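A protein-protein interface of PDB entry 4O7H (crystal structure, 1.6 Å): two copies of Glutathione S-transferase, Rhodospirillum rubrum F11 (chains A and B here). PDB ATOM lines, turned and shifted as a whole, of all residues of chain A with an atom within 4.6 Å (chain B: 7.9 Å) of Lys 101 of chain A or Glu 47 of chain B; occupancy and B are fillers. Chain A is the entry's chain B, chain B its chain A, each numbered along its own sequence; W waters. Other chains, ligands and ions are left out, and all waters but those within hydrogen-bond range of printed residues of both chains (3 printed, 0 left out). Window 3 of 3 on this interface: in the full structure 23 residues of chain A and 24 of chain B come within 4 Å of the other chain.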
ATOM      1  N   ALA A  96      19.823  18.243  22.518  1.00  0.00           N
ATOM      2  CA  ALA A  96      18.464  17.719  22.624  1.00  0.00           C
ATOM      3  C   ALA A  96      18.363  16.221  22.413  1.00  0.00           C
ATOM      4  O   ALA A  96      17.576  15.564  23.095  1.00  0.00           O
ATOM      5  CB  ALA A  96      17.530  18.441  21.663  1.00  0.00           C
ATOM      6  N   TRP A  97      19.117  15.632  21.488  1.00  0.00           N
ATOM      7  CA  TRP A  97      19.117  14.194  21.307  1.00  0.00           C
ATOM      8  C   TRP A  97      19.356  13.508  22.647  1.00  0.00           C
ATOM      9  O   TRP A  97      18.633  12.575  23.030  1.00  0.00           O
ATOM     10  CB  TRP A  97      20.208  13.766  20.306  1.00  0.00           C
ATOM     11  CG  TRP A  97      20.289  12.314  20.115  1.00  0.00           C
ATOM     12  CD1 TRP A  97      20.897  11.418  20.951  1.00  0.00           C
ATOM     13  CD2 TRP A  97      19.671  11.548  19.078  1.00  0.00           C
ATOM     14  NE1 TRP A  97      20.757  10.161  20.464  1.00  0.00           N
ATOM     15  CE2 TRP A  97      19.976  10.196  19.333  1.00  0.00           C
ATOM     16  CE3 TRP A  97      18.906  11.865  17.960  1.00  0.00           C
ATOM     17  CZ2 TRP A  97      19.576   9.190  18.504  1.00  0.00           C
ATOM     18  CZ3 TRP A  97      18.491  10.852  17.130  1.00  0.00           C
ATOM     19  CH2 TRP A  97      18.814   9.520  17.434  1.00  0.00           C
ATOM     20  N   PHE A  98      20.344  14.008  23.383  1.00  0.00           N
ATOM     21  CA  PHE A  98      20.694  13.380  24.668  1.00  0.00           C
ATOM     22  C   PHE A  98      19.781  13.785  25.793  1.00  0.00           C
ATOM     23  O   PHE A  98      19.375  12.930  26.581  1.00  0.00           O
ATOM     24  CB  PHE A  98      22.212  13.539  24.986  1.00  0.00           C
ATOM     25  CG  PHE A  98      23.045  12.702  24.064  1.00  0.00           C
ATOM     26  CD1 PHE A  98      23.208  11.334  24.279  1.00  0.00           C
ATOM     27  CD2 PHE A  98      23.548  13.245  22.903  1.00  0.00           C
ATOM     28  CE1 PHE A  98      23.915  10.566  23.353  1.00  0.00           C
ATOM     29  CE2 PHE A  98      24.239  12.468  22.010  1.00  0.00           C
ATOM     30  CZ  PHE A  98      24.397  11.138  22.216  1.00  0.00           C
ATOM     31  N   ASP A  99      19.486  15.075  25.908  1.00  0.00           N
ATOM     32  CA  ASP A  99      18.640  15.523  27.046  1.00  0.00           C
ATOM     33  C   ASP A  99      17.156  15.157  26.890  1.00  0.00           C
ATOM     34  O   ASP A  99      16.405  15.173  27.895  1.00  0.00           O
ATOM     35  CB  ASP A  99      18.775  17.044  27.281  1.00  0.00           C
ATOM     36  CG  ASP A  99      20.004  17.429  28.063  1.00  0.00           C
ATOM     37  OD1 ASP A  99      20.624  16.591  28.789  1.00  0.00           O
ATOM     38  OD2 ASP A  99      20.428  18.605  27.913  1.00  0.00           O
ATOM     39  N   ARG A 100      16.706  14.833  25.675  1.00  0.00           N
ATOM     40  CA  ARG A 100      15.337  14.296  25.438  1.00  0.00           C
ATOM     41  C   ARG A 100      15.312  12.811  25.179  1.00  0.00           C
ATOM     42  O   ARG A 100      14.778  12.035  26.004  1.00  0.00           O
ATOM     43  CB  ARG A 100      14.616  15.044  24.308  1.00  0.00           C
ATOM     44  CG  ARG A 100      13.242  14.465  23.982  1.00  0.00           C
ATOM     45  CD  ARG A 100      12.366  15.369  23.098  1.00  0.00           C
ATOM     46  NE  ARG A 100      13.101  15.714  21.905  1.00  0.00           N
ATOM     47  CZ  ARG A 100      13.506  16.929  21.576  1.00  0.00           C
ATOM     48  NH1 ARG A 100      13.238  17.981  22.367  1.00  0.00           N
ATOM     49  NH2 ARG A 100      14.210  17.080  20.470  1.00  0.00           N
ATOM     50  N   LYS A 101      15.849  12.383  24.043  1.00  0.00           N
ATOM     51  CA  LYS A 101      15.717  11.026  23.598  1.00  0.00           C
ATOM     52  C   LYS A 101      16.537  10.040  24.468  1.00  0.00           C
ATOM     53  O   LYS A 101      16.017   9.052  25.008  1.00  0.00           O
ATOM     54  CB  LYS A 101      16.067  10.895  22.105  1.00  0.00           C
ATOM     55  CG  LYS A 101      15.751   9.546  21.546  1.00  0.00           C
ATOM     56  CD  LYS A 101      16.150   9.389  20.089  1.00  0.00           C
ATOM     57  CE  LYS A 101      16.093   7.972  19.578  1.00  0.00           C
ATOM     58  NZ  LYS A 101      14.721   7.411  19.464  1.00  0.00           N
ATOM     59  N   PHE A 102      17.848  10.244  24.568  1.00  0.00           N
ATOM     60  CA  PHE A 102      18.640   9.357  25.442  1.00  0.00           C
ATOM     61  C   PHE A 102      18.097   9.401  26.851  1.00  0.00           C
ATOM     62  O   PHE A 102      17.954   8.353  27.517  1.00  0.00           O
ATOM     63  CB  PHE A 102      20.094   9.787  25.433  1.00  0.00           C
ATOM     64  CG  PHE A 102      21.024   8.854  26.133  1.00  0.00           C
ATOM     65  CD1 PHE A 102      21.121   8.843  27.521  1.00  0.00           C
ATOM     66  CD2 PHE A 102      21.878   8.052  25.407  1.00  0.00           C
ATOM     67  CE1 PHE A 102      21.993   7.984  28.166  1.00  0.00           C
ATOM     68  CE2 PHE A 102      22.748   7.209  26.033  1.00  0.00           C
ATOM     69  CZ  PHE A 102      22.796   7.176  27.413  1.00  0.00           C
ATOM     70  N   ASN A 103      17.758  10.591  27.316  1.00  0.00           N
ATOM     71  CA  ASN A 103      17.249  10.739  28.668  1.00  0.00           C
ATOM     72  C   ASN A 103      15.967   9.906  28.910  1.00  0.00           C
ATOM     73  O   ASN A 103      15.866   9.223  29.944  1.00  0.00           O
ATOM     74  CB  ASN A 103      16.995  12.220  28.988  1.00  0.00           C
ATOM     75  CG  ASN A 103      16.566  12.405  30.406  1.00  0.00           C
ATOM     76  OD1 ASN A 103      17.326  12.149  31.340  1.00  0.00           O
ATOM     77  ND2 ASN A 103      15.290  12.823  30.579  1.00  0.00           N
ATOM     78  N   ARG A 104      15.021   9.943  27.969  1.00  0.00           N
ATOM     79  CA  ARG A 104      13.756   9.219  28.151  1.00  0.00           C
ATOM     80  C   ARG A 104      13.968   7.688  28.033  1.00  0.00           C
ATOM     81  O   ARG A 104      13.326   6.905  28.738  1.00  0.00           O
ATOM     82  CB  ARG A 104      12.746   9.703  27.097  1.00  0.00           C
ATOM     83  CG  ARG A 104      11.316   9.141  27.272  1.00  0.00           C
ATOM     84  CD  ARG A 104      10.343   9.565  26.153  1.00  0.00           C
ATOM     85  NE  ARG A 104      11.104   9.689  24.915  1.00  0.00           N
ATOM     86  CZ  ARG A 104      11.219  10.787  24.147  1.00  0.00           C
ATOM     87  NH1 ARG A 104      10.511  11.911  24.385  1.00  0.00           N
ATOM     88  NH2 ARG A 104      12.048  10.728  23.101  1.00  0.00           N
ATOM     89  N   GLU A 105      14.859   7.294  27.139  1.00  0.00           N
ATOM     90  CA  GLU A 105      15.019   5.888  26.747  1.00  0.00           C
ATOM     91  C   GLU A 105      15.969   5.132  27.637  1.00  0.00           C
ATOM     92  O   GLU A 105      15.897   3.883  27.665  1.00  0.00           O
ATOM     93  CB  GLU A 105      15.478   5.785  25.278  1.00  0.00           C
ATOM     94  CG  GLU A 105      14.427   6.270  24.306  1.00  0.00           C
ATOM     95  CD  GLU A 105      14.812   6.238  22.844  1.00  0.00           C
ATOM     96  OE1 GLU A 105      15.962   5.903  22.493  1.00  0.00           O
ATOM     97  OE2 GLU A 105      13.928   6.587  22.009  1.00  0.00           O
ATOM     98  N   HIS A 140      21.959   4.134  20.986  1.00  0.00           N
ATOM     99  CA  HIS A 140      22.624   5.412  21.180  1.00  0.00           C
ATOM    100  C   HIS A 140      24.120   5.347  21.033  1.00  0.00           C
ATOM    101  O   HIS A 140      24.741   6.249  20.465  1.00  0.00           O
ATOM    102  CB  HIS A 140      22.244   6.002  22.528  1.00  0.00           C
ATOM    103  CG  HIS A 140      20.854   6.549  22.512  1.00  0.00           C
ATOM    104  ND1 HIS A 140      19.724   5.866  22.905  1.00  0.00           N
ATOM    105  CD2 HIS A 140      20.436   7.756  22.066  1.00  0.00           C
ATOM    106  CE1 HIS A 140      18.655   6.640  22.709  1.00  0.00           C
ATOM    107  NE2 HIS A 140      19.073   7.777  22.169  1.00  0.00           N
ATOM    108  N   THR B  34       4.439  12.029  12.257  1.00  0.00           N
ATOM    109  CA  THR B  34       5.639  11.318  12.667  1.00  0.00           C
ATOM    110  C   THR B  34       5.339   9.940  13.272  1.00  0.00           C
ATOM    111  O   THR B  34       6.256   9.143  13.514  1.00  0.00           O
ATOM    112  CB  THR B  34       6.465  12.168  13.655  1.00  0.00           C
ATOM    113  OG1 THR B  34       5.603  12.703  14.688  1.00  0.00           O
ATOM    114  CG2 THR B  34       7.068  13.354  12.919  1.00  0.00           C
ATOM    115  N   PHE B  41      12.076  11.122   5.902  1.00  0.00           N
ATOM    116  CA  PHE B  41      12.007  12.108   7.003  1.00  0.00           C
ATOM    117  C   PHE B  41      13.060  11.791   8.054  1.00  0.00           C
ATOM    118  O   PHE B  41      13.761  12.686   8.508  1.00  0.00           O
ATOM    119  CB  PHE B  41      10.607  12.180   7.616  1.00  0.00           C
ATOM    120  CG  PHE B  41      10.477  13.219   8.686  1.00  0.00           C
ATOM    121  CD1 PHE B  41      10.198  14.507   8.371  1.00  0.00           C
ATOM    122  CD2 PHE B  41      10.646  12.891  10.018  1.00  0.00           C
ATOM    123  CE1 PHE B  41      10.122  15.474   9.353  1.00  0.00           C
ATOM    124  CE2 PHE B  41      10.533  13.860  11.009  1.00  0.00           C
ATOM    125  CZ  PHE B  41      10.339  15.143  10.665  1.00  0.00           C
ATOM    126  N   LEU B  42      13.200  10.510   8.393  1.00  0.00           N
ATOM    127  CA  LEU B  42      14.210  10.059   9.326  1.00  0.00           C
ATOM    128  C   LEU B  42      15.601  10.373   8.839  1.00  0.00           C
ATOM    129  O   LEU B  42      16.491  10.692   9.621  1.00  0.00           O
ATOM    130  CB  LEU B  42      14.113   8.531   9.537  1.00  0.00           C
ATOM    131  CG  LEU B  42      13.116   8.064  10.564  1.00  0.00           C
ATOM    132  CD1 LEU B  42      13.077   6.533  10.570  1.00  0.00           C
ATOM    133  CD2 LEU B  42      13.472   8.589  11.950  1.00  0.00           C
ATOM    134  N   ALA B  43      15.824  10.269   7.515  1.00  0.00           N
ATOM    135  CA  ALA B  43      17.110  10.621   6.966  1.00  0.00           C
ATOM    136  C   ALA B  43      17.437  12.075   7.224  1.00  0.00           C
ATOM    137  O   ALA B  43      18.569  12.409   7.462  1.00  0.00           O
ATOM    138  CB  ALA B  43      17.187  10.331   5.455  1.00  0.00           C
ATOM    139  N   MET B  44      16.430  12.939   7.161  1.00  0.00           N
ATOM    140  CA  MET B  44      16.627  14.361   7.412  1.00  0.00           C
ATOM    141  C   MET B  44      16.790  14.684   8.919  1.00  0.00           C
ATOM    142  O   MET B  44      17.648  15.502   9.297  1.00  0.00           O
ATOM    143  CB  MET B  44      15.420  15.117   6.857  1.00  0.00           C
ATOM    144  CG  MET B  44      15.430  16.587   7.155  1.00  0.00           C
ATOM    145  SD  MET B  44      14.014  17.444   6.471  1.00  0.00           S
ATOM    146  CE  MET B  44      12.709  16.710   7.361  1.00  0.00           C
ATOM    147  N   ASN B  45      15.973  14.025   9.742  1.00  0.00           N
ATOM    148  CA  ASN B  45      16.018  14.108  11.202  1.00  0.00           C
ATOM    149  C   ASN B  45      15.963  12.770  11.885  1.00  0.00           C
ATOM    150  O   ASN B  45      14.922  12.135  12.023  1.00  0.00           O
ATOM    151  CB  ASN B  45      14.835  14.930  11.753  1.00  0.00           C
ATOM    152  CG  ASN B  45      14.898  14.999  13.255  1.00  0.00           C
ATOM    153  OD1 ASN B  45      15.912  14.653  13.817  1.00  0.00           O
ATOM    154  ND2 ASN B  45      13.868  15.494  13.905  1.00  0.00           N
ATOM    155  N   PRO B  46      17.127  12.260  12.275  1.00  0.00           N
ATOM    156  CA  PRO B  46      17.149  10.929  12.871  1.00  0.00           C
ATOM    157  C   PRO B  46      16.355  10.729  14.116  1.00  0.00           C
ATOM    158  O   PRO B  46      16.053   9.585  14.472  1.00  0.00           O
ATOM    159  CB  PRO B  46      18.626  10.705  13.142  1.00  0.00           C
ATOM    160  CG  PRO B  46      19.183  12.039  13.347  1.00  0.00           C
ATOM    161  CD  PRO B  46      18.446  12.889  12.311  1.00  0.00           C
ATOM    162  N   GLU B  47      15.995  11.823  14.812  1.00  0.00           N
ATOM    163  CA  GLU B  47      15.142  11.715  15.963  1.00  0.00           C
ATOM    164  C   GLU B  47      13.680  11.420  15.593  1.00  0.00           C
ATOM    165  O   GLU B  47      12.905  10.942  16.411  1.00  0.00           O
ATOM    166  CB  GLU B  47      15.267  12.987  16.809  1.00  0.00           C
ATOM    167  CG  GLU B  47      14.833  12.714  18.225  1.00  0.00           C
ATOM    168  CD  GLU B  47      14.739  13.925  19.148  1.00  0.00           C
ATOM    169  OE1 GLU B  47      15.210  15.055  18.820  1.00  0.00           O
ATOM    170  OE2 GLU B  47      14.222  13.692  20.251  1.00  0.00           O
ATOM    171  N   GLY B  48      13.309  11.695  14.346  1.00  0.00           N
ATOM    172  CA  GLY B  48      11.973  11.389  13.808  1.00  0.00           C
ATOM    173  C   GLY B  48      10.878  12.238  14.418  1.00  0.00           C
ATOM    174  O   GLY B  48       9.720  11.793  14.523  1.00  0.00           O
ATOM    175  N   GLU B  49      11.250  13.457  14.813  1.00  0.00           N
ATOM    176  CA  GLU B  49      10.299  14.402  15.380  1.00  0.00           C
ATOM    177  C   GLU B  49      10.159  15.633  14.515  1.00  0.00           C
ATOM    178  O   GLU B  49      11.102  16.005  13.814  1.00  0.00           O
ATOM    179  CB  GLU B  49      10.790  14.872  16.738  1.00  0.00           C
ATOM    180  CG  GLU B  49      11.113  13.762  17.733  1.00  0.00           C
ATOM    181  CD  GLU B  49       9.951  13.275  18.538  1.00  0.00           C
ATOM    182  OE1 GLU B  49       8.760  13.541  18.147  1.00  0.00           O
ATOM    183  OE2 GLU B  49      10.240  12.632  19.605  1.00  0.00           O
ATOM    184  N   VAL B  50       8.993  16.282  14.633  1.00  0.00           N
ATOM    185  CA  VAL B  50       8.843  17.662  14.259  1.00  0.00           C
ATOM    186  C   VAL B  50       9.060  18.578  15.500  1.00  0.00           C
ATOM    187  O   VAL B  50       8.847  18.135  16.631  1.00  0.00           O
ATOM    188  CB  VAL B  50       7.476  17.964  13.624  1.00  0.00           C
ATOM    189  CG1 VAL B  50       7.376  17.242  12.282  1.00  0.00           C
ATOM    190  CG2 VAL B  50       6.333  17.581  14.574  1.00  0.00           C
ATOM    191  N   PRO B  51       9.442  19.840  15.293  1.00  0.00           N
ATOM    192  CA  PRO B  51       9.665  20.585  14.042  1.00  0.00           C
ATOM    193  C   PRO B  51      11.034  20.415  13.435  1.00  0.00           C
ATOM    194  O   PRO B  51      12.039  20.116  14.121  1.00  0.00           O
ATOM    195  CB  PRO B  51       9.498  22.039  14.452  1.00  0.00           C
ATOM    196  CG  PRO B  51       9.955  22.051  15.892  1.00  0.00           C
ATOM    197  CD  PRO B  51       9.555  20.731  16.471  1.00  0.00           C
ATOM    198  N   THR B  62      17.071  21.288  13.318  1.00  0.00           N
ATOM    199  CA  THR B  62      16.215  20.290  13.963  1.00  0.00           C
ATOM    200  C   THR B  62      16.183  20.585  15.475  1.00  0.00           C
ATOM    201  O   THR B  62      17.203  21.006  16.038  1.00  0.00           O
ATOM    202  CB  THR B  62      16.859  18.921  13.695  1.00  0.00           C
ATOM    203  OG1 THR B  62      16.851  18.639  12.276  1.00  0.00           O
ATOM    204  CG2 THR B  62      16.221  17.887  14.436  1.00  0.00           C
ATOM    205  N   ASP B  63      15.051  20.338  16.113  1.00  0.00           N
ATOM    206  CA  ASP B  63      14.781  20.522  17.532  1.00  0.00           C
ATOM    207  C   ASP B  63      14.215  21.917  17.753  1.00  0.00           C
ATOM    208  O   ASP B  63      14.763  22.907  17.270  1.00  0.00           O
ATOM    209  CB  ASP B  63      15.990  20.364  18.488  1.00  0.00           C
ATOM    210  CG  ASP B  63      15.624  20.708  19.913  1.00  0.00           C
ATOM    211  OD1 ASP B  63      14.846  19.961  20.519  1.00  0.00           O
ATOM    212  OD2 ASP B  63      16.133  21.706  20.438  1.00  0.00           O
ATOM    213  N   GLY B  64      13.096  21.986  18.469  1.00  0.00           N
ATOM    214  CA  GLY B  64      12.441  23.271  18.733  1.00  0.00           C
ATOM    215  C   GLY B  64      13.375  24.312  19.344  1.00  0.00           C
ATOM    216  O   GLY B  64      13.367  25.485  18.944  1.00  0.00           O
HETATM  217  O   HOH W   1      12.555  11.741  20.606  1.00  0.00           O
HETATM  218  O   HOH W   2      14.802   7.994  16.268  1.00  0.00           O
HETATM  219  O   HOH W   3      12.851   9.556  18.802  1.00  0.00           O
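Of the 11 printed residues of chain A, 4 touch a printed residue of chain B.
Hydrophobic or aromatic side chains of chain B that line the printed part of chain A: Pro 46.
Among the printed residues, 6 pairs touch across the chains.
No position is printed for both chains.
Of the 6 pairs that touch across the chains among the printed residues, none has its exchanged pair printed and touching as well.
Among the printed residues, pairs that only touch across the chains: Ala 96 of chain A with Asp 63 of chain B (3.3 Å), Trp 97 of chain A with Glu 47 of chain B (3.5 Å), Trp 97 of chain A with Pro 46 of chain B (3.7 Å) and Lys 101 of chain A with Glu 47 of chain B (3.8 Å).
N of Phe 102 of chain A is in hydrogen-bond range of O of Trp 97 of chain A, 2.9 Å away.
NE1 of Trp 97 of chain A lies close to NE2 of His 140 of chain A (3.4 Å).
OD1 of Asn 45 of chain B is in hydrogen-bond range of N of Glu 47 of chain B (3.0 Å).
NZ of Lys 101 of chain A lies within salt-bridge range of OE2 of Glu 105 of chain A (2.8 Å).
Water W1 lies within hydrogen-bond range of the side-chain carboxylate of Glu 47 of chain B (2.6 Å), the side-chain carboxylate of Glu 49 of chain B (2.7 Å) and the guanidinium group of Arg 104 of chain A (2.7 Å).
Water W2 bridges O of Pro 46 of chain B and NZ of Lys 101 of chain A.
Water W3 lies within hydrogen-bond range of the backbone carbonyl oxygen (O) of Glu 47 of chain B and the side-chain amino group (NZ) of Lys 101 of chain A.
Glu 47 of chain B touches three residues of chain A.
Of the printed residues of chain B, Trp 97 of chain A touches Pro 46 and Glu 47.
Printed residues of chain A within 4 Å of Pro 46 of chain B: Trp 97.
Printed residues of chain B within 4 Å of Ala 96 of chain A: Asp 63 (3.3 Å).
Of the printed residues of chain A, Asp 63 of chain B touches Ala 96 (3.3 Å) and Arg 100 (3.0 Å).
Pro 51 of chain B touches none of the printed residues of chain A.
Val 50 of chain B touches none of the printed residues of chain A.
The nearest residue of chain B that does not touch Lys 101 of chain A is Pro 46 of chain B (5.4 Å).
The nearest printed residue of chain A that does not touch Glu 47 of chain B is Arg 104 of chain A (4.7 Å).
The nearest printed residue of chain A that does not touch Pro 46 of chain B is Lys 101 of chain A (5.4 Å).
OD1 of Asp 63 of chain B lies within salt-bridge range of NH2 of Arg 100 of chain A (3.0 Å).
The side-chain carboxylate of Glu 47 of chain B is in salt-bridge range of the guanidinium group of Arg 100 of chain A (2.8 Å).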
